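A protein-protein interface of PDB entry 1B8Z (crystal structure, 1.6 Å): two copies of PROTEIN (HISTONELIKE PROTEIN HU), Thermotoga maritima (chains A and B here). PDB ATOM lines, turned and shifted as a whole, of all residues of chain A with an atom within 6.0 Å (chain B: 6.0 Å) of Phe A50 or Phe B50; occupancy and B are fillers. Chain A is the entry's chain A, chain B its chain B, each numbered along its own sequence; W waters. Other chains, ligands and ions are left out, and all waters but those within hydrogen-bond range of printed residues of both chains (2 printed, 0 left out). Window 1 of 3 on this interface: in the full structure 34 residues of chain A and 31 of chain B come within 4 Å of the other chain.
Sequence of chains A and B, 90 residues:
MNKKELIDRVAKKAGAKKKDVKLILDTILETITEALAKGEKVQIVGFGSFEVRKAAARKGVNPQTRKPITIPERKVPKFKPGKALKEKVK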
ATOM      1  N   ILE A  32     -21.861 -14.768  22.374  1.00  0.00           N
ATOM      2  CA  ILE A  32     -20.453 -14.706  22.726  1.00  0.00           C
ATOM      3  C   ILE A  32     -20.293 -14.166  24.147  1.00  0.00           C
ATOM      4  O   ILE A  32     -19.532 -14.731  24.953  1.00  0.00           O
ATOM      5  CB  ILE A  32     -19.669 -13.824  21.717  1.00  0.00           C
ATOM      6  CG1 ILE A  32     -19.677 -14.523  20.372  1.00  0.00           C
ATOM      7  CG2 ILE A  32     -18.263 -13.515  22.241  1.00  0.00           C
ATOM      8  CD1 ILE A  32     -19.095 -13.651  19.242  1.00  0.00           C
ATOM      9  N   LEU A  36     -18.570 -16.197  27.368  1.00  0.00           N
ATOM     10  CA  LEU A  36     -17.440 -15.628  28.090  1.00  0.00           C
ATOM     11  C   LEU A  36     -17.768 -15.435  29.573  1.00  0.00           C
ATOM     12  O   LEU A  36     -16.890 -15.644  30.423  1.00  0.00           O
ATOM     13  CB  LEU A  36     -17.005 -14.288  27.493  1.00  0.00           C
ATOM     14  CG  LEU A  36     -16.426 -14.409  26.075  1.00  0.00           C
ATOM     15  CD1 LEU A  36     -16.064 -13.016  25.568  1.00  0.00           C
ATOM     16  CD2 LEU A  36     -15.240 -15.336  25.988  1.00  0.00           C
ATOM     17  N   GLU A  40     -16.306 -19.874  29.102  1.00  0.00           N
ATOM     18  CA  GLU A  40     -16.121 -20.698  27.922  1.00  0.00           C
ATOM     19  C   GLU A  40     -15.311 -19.909  26.887  1.00  0.00           C
ATOM     20  O   GLU A  40     -15.224 -18.676  26.946  1.00  0.00           O
ATOM     21  CB  GLU A  40     -17.475 -21.090  27.333  1.00  0.00           C
ATOM     22  CG  GLU A  40     -17.463 -22.199  26.313  1.00  0.00           C
ATOM     23  CD  GLU A  40     -18.857 -22.639  25.895  1.00  0.00           C
ATOM     24  OE1 GLU A  40     -19.833 -22.097  26.458  1.00  0.00           O
ATOM     25  OE2 GLU A  40     -18.919 -23.531  25.017  1.00  0.00           O
ATOM     26  N   LYS A  41     -14.706 -20.613  25.962  1.00  0.00           N
ATOM     27  CA  LYS A  41     -13.959 -20.001  24.863  1.00  0.00           C
ATOM     28  C   LYS A  41     -14.889 -19.972  23.655  1.00  0.00           C
ATOM     29  O   LYS A  41     -15.804 -20.801  23.559  1.00  0.00           O
ATOM     30  CB  LYS A  41     -12.805 -20.960  24.582  1.00  0.00           C
ATOM     31  CG  LYS A  41     -11.729 -20.617  23.595  1.00  0.00           C
ATOM     32  CD  LYS A  41     -10.601 -21.645  23.712  1.00  0.00           C
ATOM     33  N   VAL A  42     -14.747 -18.966  22.792  1.00  0.00           N
ATOM     34  CA  VAL A  42     -15.517 -18.945  21.544  1.00  0.00           C
ATOM     35  C   VAL A  42     -14.471 -18.924  20.436  1.00  0.00           C
ATOM     36  O   VAL A  42     -13.846 -17.878  20.179  1.00  0.00           O
ATOM     37  CB  VAL A  42     -16.535 -17.808  21.374  1.00  0.00           C
ATOM     38  CG1 VAL A  42     -17.232 -17.924  20.029  1.00  0.00           C
ATOM     39  CG2 VAL A  42     -17.525 -17.847  22.539  1.00  0.00           C
ATOM     40  N   GLN A  43     -14.270 -20.041  19.769  1.00  0.00           N
ATOM     41  CA  GLN A  43     -13.245 -20.179  18.743  1.00  0.00           C
ATOM     42  C   GLN A  43     -13.872 -20.210  17.373  1.00  0.00           C
ATOM     43  O   GLN A  43     -14.714 -21.058  17.094  1.00  0.00           O
ATOM     44  CB  GLN A  43     -12.457 -21.482  18.983  1.00  0.00           C
ATOM     45  CG  GLN A  43     -11.177 -21.504  18.137  1.00  0.00           C
ATOM     46  CD  GLN A  43      -9.974 -21.956  18.942  1.00  0.00           C
ATOM     47  OE1 GLN A  43     -10.106 -22.648  19.953  1.00  0.00           O
ATOM     48  NE2 GLN A  43      -8.782 -21.580  18.492  1.00  0.00           N
ATOM     49  N   ILE A  44     -13.529 -19.190  16.558  1.00  0.00           N
ATOM     50  CA  ILE A  44     -14.129 -19.149  15.226  1.00  0.00           C
ATOM     51  C   ILE A  44     -13.019 -19.387  14.206  1.00  0.00           C
ATOM     52  O   ILE A  44     -12.196 -18.494  13.984  1.00  0.00           O
ATOM     53  CB  ILE A  44     -14.808 -17.788  14.953  1.00  0.00           C
ATOM     54  CG1 ILE A  44     -15.901 -17.551  15.992  1.00  0.00           C
ATOM     55  CG2 ILE A  44     -15.355 -17.775  13.534  1.00  0.00           C
ATOM     56  CD1 ILE A  44     -16.434 -16.125  16.044  1.00  0.00           C
ATOM     57  N   PHE A  47     -10.900 -16.772  11.892  1.00  0.00           N
ATOM     58  CA  PHE A  47     -11.094 -15.433  12.436  1.00  0.00           C
ATOM     59  C   PHE A  47     -10.294 -15.274  13.706  1.00  0.00           C
ATOM     60  O   PHE A  47      -9.338 -14.483  13.781  1.00  0.00           O
ATOM     61  CB  PHE A  47     -12.579 -15.091  12.606  1.00  0.00           C
ATOM     62  CG  PHE A  47     -12.794 -13.648  12.973  1.00  0.00           C
ATOM     63  CD1 PHE A  47     -12.662 -12.644  12.026  1.00  0.00           C
ATOM     64  CD2 PHE A  47     -13.133 -13.313  14.267  1.00  0.00           C
ATOM     65  CE1 PHE A  47     -12.867 -11.326  12.389  1.00  0.00           C
ATOM     66  CE2 PHE A  47     -13.334 -11.989  14.635  1.00  0.00           C
ATOM     67  CZ  PHE A  47     -13.201 -10.997  13.685  1.00  0.00           C
ATOM     68  N   GLY A  48     -10.635 -16.024  14.761  1.00  0.00           N
ATOM     69  CA  GLY A  48      -9.897 -15.923  16.007  1.00  0.00           C
ATOM     70  C   GLY A  48     -10.723 -16.479  17.159  1.00  0.00           C
ATOM     71  O   GLY A  48     -11.813 -16.990  16.947  1.00  0.00           O
ATOM     72  N   SER A  49     -10.165 -16.372  18.360  1.00  0.00           N
ATOM     73  CA  SER A  49     -10.877 -16.892  19.518  1.00  0.00           C
ATOM     74  C   SER A  49     -11.075 -15.818  20.568  1.00  0.00           C
ATOM     75  O   SER A  49     -10.221 -14.945  20.765  1.00  0.00           O
ATOM     76  CB  SER A  49     -10.095 -18.080  20.108  1.00  0.00           C
ATOM     77  OG  SER A  49      -8.769 -17.656  20.357  1.00  0.00           O
ATOM     78  N   PHE A  50     -12.224 -15.882  21.222  1.00  0.00           N
ATOM     79  CA  PHE A  50     -12.517 -14.979  22.335  1.00  0.00           C
ATOM     80  C   PHE A  50     -12.388 -15.834  23.602  1.00  0.00           C
ATOM     81  O   PHE A  50     -12.915 -16.946  23.614  1.00  0.00           O
ATOM     82  CB  PHE A  50     -13.936 -14.433  22.270  1.00  0.00           C
ATOM     83  CG  PHE A  50     -14.176 -13.508  21.108  1.00  0.00           C
ATOM     84  CD1 PHE A  50     -14.550 -13.998  19.876  1.00  0.00           C
ATOM     85  CD2 PHE A  50     -13.969 -12.146  21.283  1.00  0.00           C
ATOM     86  CE1 PHE A  50     -14.764 -13.134  18.812  1.00  0.00           C
ATOM     87  CE2 PHE A  50     -14.175 -11.279  20.219  1.00  0.00           C
ATOM     88  CZ  PHE A  50     -14.577 -11.774  19.004  1.00  0.00           C
ATOM     89  N   GLU A  51     -11.690 -15.331  24.606  1.00  0.00           N
ATOM     90  CA  GLU A  51     -11.508 -16.123  25.826  1.00  0.00           C
ATOM     91  C   GLU A  51     -11.401 -15.150  26.995  1.00  0.00           C
ATOM     92  O   GLU A  51     -11.316 -13.932  26.808  1.00  0.00           O
ATOM     93  CB  GLU A  51     -10.269 -17.005  25.710  1.00  0.00           C
ATOM     94  CG  GLU A  51      -8.960 -16.224  25.646  1.00  0.00           C
ATOM     95  CD  GLU A  51      -7.763 -17.120  25.330  1.00  0.00           C
ATOM     96  OE1 GLU A  51      -7.941 -18.378  25.105  1.00  0.00           O
ATOM     97  OE2 GLU A  51      -6.579 -16.618  25.285  1.00  0.00           O
ATOM     98  N   VAL A  52     -11.435 -15.685  28.192  1.00  0.00           N
ATOM     99  CA  VAL A  52     -11.280 -14.858  29.392  1.00  0.00           C
ATOM    100  C   VAL A  52      -9.995 -15.283  30.098  1.00  0.00           C
ATOM    101  O   VAL A  52      -9.662 -16.478  30.141  1.00  0.00           O
ATOM    102  CB  VAL A  52     -12.492 -15.000  30.324  1.00  0.00           C
ATOM    103  CG1 VAL A  52     -12.337 -14.204  31.627  1.00  0.00           C
ATOM    104  CG2 VAL A  52     -13.797 -14.501  29.695  1.00  0.00           C
ATOM    105  N   LYS A  78     -10.442 -11.428  26.232  1.00  0.00           N
ATOM    106  CA  LYS A  78      -9.311 -11.271  25.336  1.00  0.00           C
ATOM    107  C   LYS A  78      -9.645 -11.912  23.991  1.00  0.00           C
ATOM    108  O   LYS A  78     -10.381 -12.899  23.945  1.00  0.00           O
ATOM    109  CB  LYS A  78      -8.046 -11.950  25.873  1.00  0.00           C
ATOM    110  N   PHE A  79      -9.080 -11.376  22.924  1.00  0.00           N
ATOM    111  CA  PHE A  79      -9.249 -11.906  21.584  1.00  0.00           C
ATOM    112  C   PHE A  79      -7.885 -12.279  21.021  1.00  0.00           C
ATOM    113  O   PHE A  79      -6.954 -11.463  21.017  1.00  0.00           O
ATOM    114  CB  PHE A  79      -9.916 -10.882  20.653  1.00  0.00           C
ATOM    115  CG  PHE A  79     -10.026 -11.287  19.216  1.00  0.00           C
ATOM    116  CD1 PHE A  79     -10.941 -12.230  18.798  1.00  0.00           C
ATOM    117  CD2 PHE A  79      -9.197 -10.705  18.263  1.00  0.00           C
ATOM    118  CE1 PHE A  79     -11.059 -12.603  17.465  1.00  0.00           C
ATOM    119  CE2 PHE A  79      -9.305 -11.065  16.937  1.00  0.00           C
ATOM    120  CZ  PHE A  79     -10.218 -12.022  16.530  1.00  0.00           C
ATOM    121  N   LYS A  80      -7.767 -13.500  20.535  1.00  0.00           N
ATOM    122  CA  LYS A  80      -6.554 -13.981  19.894  1.00  0.00           C
ATOM    123  C   LYS A  80      -6.837 -14.187  18.406  1.00  0.00           C
ATOM    124  O   LYS A  80      -7.558 -15.120  18.018  1.00  0.00           O
ATOM    125  CB  LYS A  80      -6.094 -15.283  20.563  1.00  0.00           C
ATOM    126  N   ILE B  32     -15.723  -7.226   8.709  1.00  0.00           N
ATOM    127  CA  ILE B  32     -14.748  -6.774   9.682  1.00  0.00           C
ATOM    128  C   ILE B  32     -13.336  -6.989   9.154  1.00  0.00           C
ATOM    129  O   ILE B  32     -12.478  -6.097   9.256  1.00  0.00           O
ATOM    130  CB  ILE B  32     -14.948  -7.524  11.026  1.00  0.00           C
ATOM    131  CG1 ILE B  32     -16.280  -7.101  11.612  1.00  0.00           C
ATOM    132  CG2 ILE B  32     -13.745  -7.275  11.942  1.00  0.00           C
ATOM    133  CD1 ILE B  32     -16.652  -7.942  12.858  1.00  0.00           C
ATOM    134  N   LEU B  36     -10.445  -4.000   8.541  1.00  0.00           N
ATOM    135  CA  LEU B  36      -9.138  -4.062   9.188  1.00  0.00           C
ATOM    136  C   LEU B  36      -8.015  -4.075   8.149  1.00  0.00           C
ATOM    137  O   LEU B  36      -6.960  -3.468   8.387  1.00  0.00           O
ATOM    138  CB  LEU B  36      -9.000  -5.294  10.089  1.00  0.00           C
ATOM    139  CG  LEU B  36      -9.936  -5.241  11.307  1.00  0.00           C
ATOM    140  CD1 LEU B  36      -9.825  -6.557  12.069  1.00  0.00           C
ATOM    141  CD2 LEU B  36      -9.674  -4.046  12.182  1.00  0.00           C
ATOM    142  N   GLU B  40      -9.085   0.416   8.859  1.00  0.00           N
ATOM    143  CA  GLU B  40     -10.214   1.052   9.514  1.00  0.00           C
ATOM    144  C   GLU B  40     -10.482   0.382  10.867  1.00  0.00           C
ATOM    145  O   GLU B  40     -10.052  -0.759  11.101  1.00  0.00           O
ATOM    146  CB  GLU B  40     -11.482   1.008   8.655  1.00  0.00           C
ATOM    147  CG  GLU B  40     -11.248   1.577   7.266  1.00  0.00           C
ATOM    148  CD  GLU B  40     -12.467   1.621   6.379  1.00  0.00           C
ATOM    149  OE1 GLU B  40     -13.467   0.951   6.698  1.00  0.00           O
ATOM    150  OE2 GLU B  40     -12.394   2.344   5.352  1.00  0.00           O
ATOM    151  N   LYS B  41     -11.170   1.098  11.736  1.00  0.00           N
ATOM    152  CA  LYS B  41     -11.535   0.510  13.035  1.00  0.00           C
ATOM    153  C   LYS B  41     -12.979   0.043  12.921  1.00  0.00           C
ATOM    154  O   LYS B  41     -13.747   0.531  12.080  1.00  0.00           O
ATOM    155  CB  LYS B  41     -11.310   1.590  14.077  1.00  0.00           C
ATOM    156  CG  LYS B  41     -12.202   1.676  15.280  1.00  0.00           C
ATOM    157  CD  LYS B  41     -11.797   2.871  16.140  1.00  0.00           C
ATOM    158  CE  LYS B  41     -11.462   2.400  17.549  1.00  0.00           C
ATOM    159  NZ  LYS B  41     -10.683   3.428  18.301  1.00  0.00           N
ATOM    160  N   VAL B  42     -13.314  -1.011  13.664  1.00  0.00           N
ATOM    161  CA  VAL B  42     -14.699  -1.500  13.680  1.00  0.00           C
ATOM    162  C   VAL B  42     -15.122  -1.394  15.140  1.00  0.00           C
ATOM    163  O   VAL B  42     -14.728  -2.222  15.975  1.00  0.00           O
ATOM    164  CB  VAL B  42     -14.945  -2.907  13.123  1.00  0.00           C
ATOM    165  CG1 VAL B  42     -16.413  -3.266  13.240  1.00  0.00           C
ATOM    166  CG2 VAL B  42     -14.451  -2.953  11.676  1.00  0.00           C
ATOM    167  N   GLN B  43     -15.922  -0.396  15.457  1.00  0.00           N
ATOM    168  CA  GLN B  43     -16.338  -0.112  16.829  1.00  0.00           C
ATOM    169  C   GLN B  43     -17.773  -0.521  17.034  1.00  0.00           C
ATOM    170  O   GLN B  43     -18.658  -0.047  16.325  1.00  0.00           O
ATOM    171  CB  GLN B  43     -16.196   1.403  17.077  1.00  0.00           C
ATOM    172  CG  GLN B  43     -16.353   1.752  18.560  1.00  0.00           C
ATOM    173  CD  GLN B  43     -15.215   2.647  19.033  1.00  0.00           C
ATOM    174  OE1 GLN B  43     -14.650   3.431  18.262  1.00  0.00           O
ATOM    175  NE2 GLN B  43     -14.877   2.542  20.311  1.00  0.00           N
ATOM    176  N   ILE B  44     -18.011  -1.489  17.930  1.00  0.00           N
ATOM    177  CA  ILE B  44     -19.370  -1.963  18.146  1.00  0.00           C
ATOM    178  C   ILE B  44     -19.758  -1.591  19.575  1.00  0.00           C
ATOM    179  O   ILE B  44     -19.277  -2.210  20.524  1.00  0.00           O
ATOM    180  CB  ILE B  44     -19.483  -3.496  17.986  1.00  0.00           C
ATOM    181  CG1 ILE B  44     -19.104  -3.856  16.547  1.00  0.00           C
ATOM    182  CG2 ILE B  44     -20.888  -3.972  18.321  1.00  0.00           C
ATOM    183  CD1 ILE B  44     -18.845  -5.335  16.312  1.00  0.00           C
ATOM    184  N   PHE B  47     -19.914  -3.804  23.022  1.00  0.00           N
ATOM    185  CA  PHE B  47     -19.125  -5.008  22.817  1.00  0.00           C
ATOM    186  C   PHE B  47     -17.644  -4.700  22.809  1.00  0.00           C
ATOM    187  O   PHE B  47     -16.903  -5.134  23.707  1.00  0.00           O
ATOM    188  CB  PHE B  47     -19.581  -5.785  21.581  1.00  0.00           C
ATOM    189  CG  PHE B  47     -18.918  -7.125  21.429  1.00  0.00           C
ATOM    190  CD1 PHE B  47     -19.312  -8.211  22.207  1.00  0.00           C
ATOM    191  CD2 PHE B  47     -17.925  -7.303  20.489  1.00  0.00           C
ATOM    192  CE1 PHE B  47     -18.691  -9.437  22.045  1.00  0.00           C
ATOM    193  CE2 PHE B  47     -17.298  -8.531  20.326  1.00  0.00           C
ATOM    194  CZ  PHE B  47     -17.692  -9.596  21.108  1.00  0.00           C
ATOM    195  N   GLY B  48     -17.138  -3.903  21.869  1.00  0.00           N
ATOM    196  CA  GLY B  48     -15.729  -3.578  21.822  1.00  0.00           C
ATOM    197  C   GLY B  48     -15.325  -3.104  20.438  1.00  0.00           C
ATOM    198  O   GLY B  48     -16.195  -2.972  19.580  1.00  0.00           O
ATOM    199  N   SER B  49     -14.037  -2.834  20.265  1.00  0.00           N
ATOM    200  CA  SER B  49     -13.572  -2.362  18.983  1.00  0.00           C
ATOM    201  C   SER B  49     -12.460  -3.235  18.439  1.00  0.00           C
ATOM    202  O   SER B  49     -11.624  -3.754  19.190  1.00  0.00           O
ATOM    203  CB  SER B  49     -13.085  -0.908  19.127  1.00  0.00           C
ATOM    204  OG  SER B  49     -12.083  -0.889  20.129  1.00  0.00           O
ATOM    205  N   PHE B  50     -12.489  -3.443  17.135  1.00  0.00           N
ATOM    206  CA  PHE B  50     -11.429  -4.161  16.444  1.00  0.00           C
ATOM    207  C   PHE B  50     -10.607  -3.101  15.706  1.00  0.00           C
ATOM    208  O   PHE B  50     -11.170  -2.211  15.072  1.00  0.00           O
ATOM    209  CB  PHE B  50     -11.992  -5.104  15.384  1.00  0.00           C
ATOM    210  CG  PHE B  50     -12.792  -6.242  15.969  1.00  0.00           C
ATOM    211  CD1 PHE B  50     -14.143  -6.118  16.194  1.00  0.00           C
ATOM    212  CD2 PHE B  50     -12.118  -7.405  16.315  1.00  0.00           C
ATOM    213  CE1 PHE B  50     -14.859  -7.173  16.736  1.00  0.00           C
ATOM    214  CE2 PHE B  50     -12.831  -8.466  16.861  1.00  0.00           C
ATOM    215  CZ  PHE B  50     -14.180  -8.337  17.071  1.00  0.00           C
ATOM    216  N   GLU B  51      -9.289  -3.183  15.859  1.00  0.00           N
ATOM    217  CA  GLU B  51      -8.443  -2.192  15.183  1.00  0.00           C
ATOM    218  C   GLU B  51      -7.121  -2.860  14.828  1.00  0.00           C
ATOM    219  O   GLU B  51      -6.866  -4.012  15.201  1.00  0.00           O
ATOM    220  CB  GLU B  51      -8.235  -0.972  16.069  1.00  0.00           C
ATOM    221  CG  GLU B  51      -8.037  -1.269  17.545  1.00  0.00           C
ATOM    222  CD  GLU B  51      -7.644  -0.008  18.310  1.00  0.00           C
ATOM    223  OE1 GLU B  51      -8.236   1.111  18.052  1.00  0.00           O
ATOM    224  OE2 GLU B  51      -6.716  -0.059  19.198  1.00  0.00           O
ATOM    225  N   VAL B  52      -6.302  -2.146  14.091  1.00  0.00           N
ATOM    226  CA  VAL B  52      -4.981  -2.659  13.722  1.00  0.00           C
ATOM    227  C   VAL B  52      -3.906  -1.762  14.343  1.00  0.00           C
ATOM    228  O   VAL B  52      -3.988  -0.524  14.243  1.00  0.00           O
ATOM    229  CB  VAL B  52      -4.825  -2.733  12.196  1.00  0.00           C
ATOM    230  CG1 VAL B  52      -3.445  -3.249  11.767  1.00  0.00           C
ATOM    231  CG2 VAL B  52      -5.836  -3.680  11.536  1.00  0.00           C
ATOM    232  N   LYS B  78      -6.155  -6.194  16.659  1.00  0.00           N
ATOM    233  CA  LYS B  78      -6.317  -6.118  18.096  1.00  0.00           C
ATOM    234  C   LYS B  78      -7.790  -5.870  18.427  1.00  0.00           C
ATOM    235  O   LYS B  78      -8.493  -5.218  17.657  1.00  0.00           O
ATOM    236  CB  LYS B  78      -5.486  -4.991  18.725  1.00  0.00           C
ATOM    237  N   PHE B  79      -8.243  -6.403  19.545  1.00  0.00           N
ATOM    238  CA  PHE B  79      -9.587  -6.214  20.047  1.00  0.00           C
ATOM    239  C   PHE B  79      -9.520  -5.532  21.406  1.00  0.00           C
ATOM    240  O   PHE B  79      -8.828  -5.990  22.333  1.00  0.00           O
ATOM    241  CB  PHE B  79     -10.350  -7.542  20.213  1.00  0.00           C
ATOM    242  CG  PHE B  79     -11.712  -7.414  20.823  1.00  0.00           C
ATOM    243  CD1 PHE B  79     -12.749  -6.828  20.123  1.00  0.00           C
ATOM    244  CD2 PHE B  79     -11.970  -7.878  22.107  1.00  0.00           C
ATOM    245  CE1 PHE B  79     -14.022  -6.722  20.668  1.00  0.00           C
ATOM    246  CE2 PHE B  79     -13.229  -7.772  22.667  1.00  0.00           C
ATOM    247  CZ  PHE B  79     -14.257  -7.176  21.951  1.00  0.00           C
ATOM    248  N   LYS B  80     -10.252  -4.445  21.549  1.00  0.00           N
ATOM    249  CA  LYS B  80     -10.363  -3.725  22.814  1.00  0.00           C
ATOM    250  C   LYS B  80     -11.786  -3.883  23.351  1.00  0.00           C
ATOM    251  O   LYS B  80     -12.739  -3.307  22.803  1.00  0.00           O
ATOM    252  CB  LYS B  80     -10.009  -2.241  22.626  1.00  0.00           C
HETATM  253  O   HOH W   1      -6.555  -8.607  20.719  1.00  0.00           O
HETATM  254  O   HOH W   2      -8.023  -8.653  23.403  1.00  0.00           O
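N of Phe A50 is in hydrogen-bond range of O of Val A42 (2.8 Å).
O of Val B42 lies within hydrogen-bond range of N of Phe B50 (2.8 Å).
Among the printed residues, merely in contact across the chains: Phe A79 with Phe B79 (3.4 Å), Phe A50 with Phe B50 (3.96 Å) and Phe A50 with Phe B47 (3.999 Å).
Of the printed residues of chain B, Phe A50 touches Phe B47 and Phe B50.
Phe B50 touches just one residue of chain A: Phe A50.
Of the printed residues of chain A, Phe B47 touches Phe A50 (3.999 Å).
Printed residues of chain B within 4 Å of Phe A79: Phe B79 (3.4 Å).
The nearest printed residue of chain B that does not touch Phe A50 is Phe B79 (4.4 Å).
The nearest printed residue of chain A that does not touch Phe B47 is Ile A32 (4.1 Å).
Hydrophobic or aromatic side chains of chain B that line the printed part of chain A: Phe B47, Phe B50 and Phe B79.
Hydrophobic or aromatic side chains of chain A within 4 Å of the printed part of chain B: Phe A50 and Phe A79.
Among the printed residues, 3 pairs touch across the chains.
Among the printed residues, no Asp or Glu carboxylate lies within 4 Å of a Lys or Arg side-chain nitrogen of the other chain.
Phe A50 touches Phe B47, but with the chains exchanged Phe A47 does not touch Phe B50 (4.1 Å).
Phe B50 touches its own counterpart, Phe A50.
Phe B79 touches its own counterpart, Phe A79.
Of the 3 pairs that touch across the chains among the printed residues, 2 have their exchanged pair printed and touching as well.
Water W1 lies within hydrogen-bond range of the backbone carbonyl oxygen (O) of Phe A79 (2.9 Å) and the backbone NH (N) of Phe B79 (3.0 Å).
Water W2 lies within hydrogen-bond range of N of Phe A79 (3.0 Å) and O of Phe B79 (3.0 Å).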
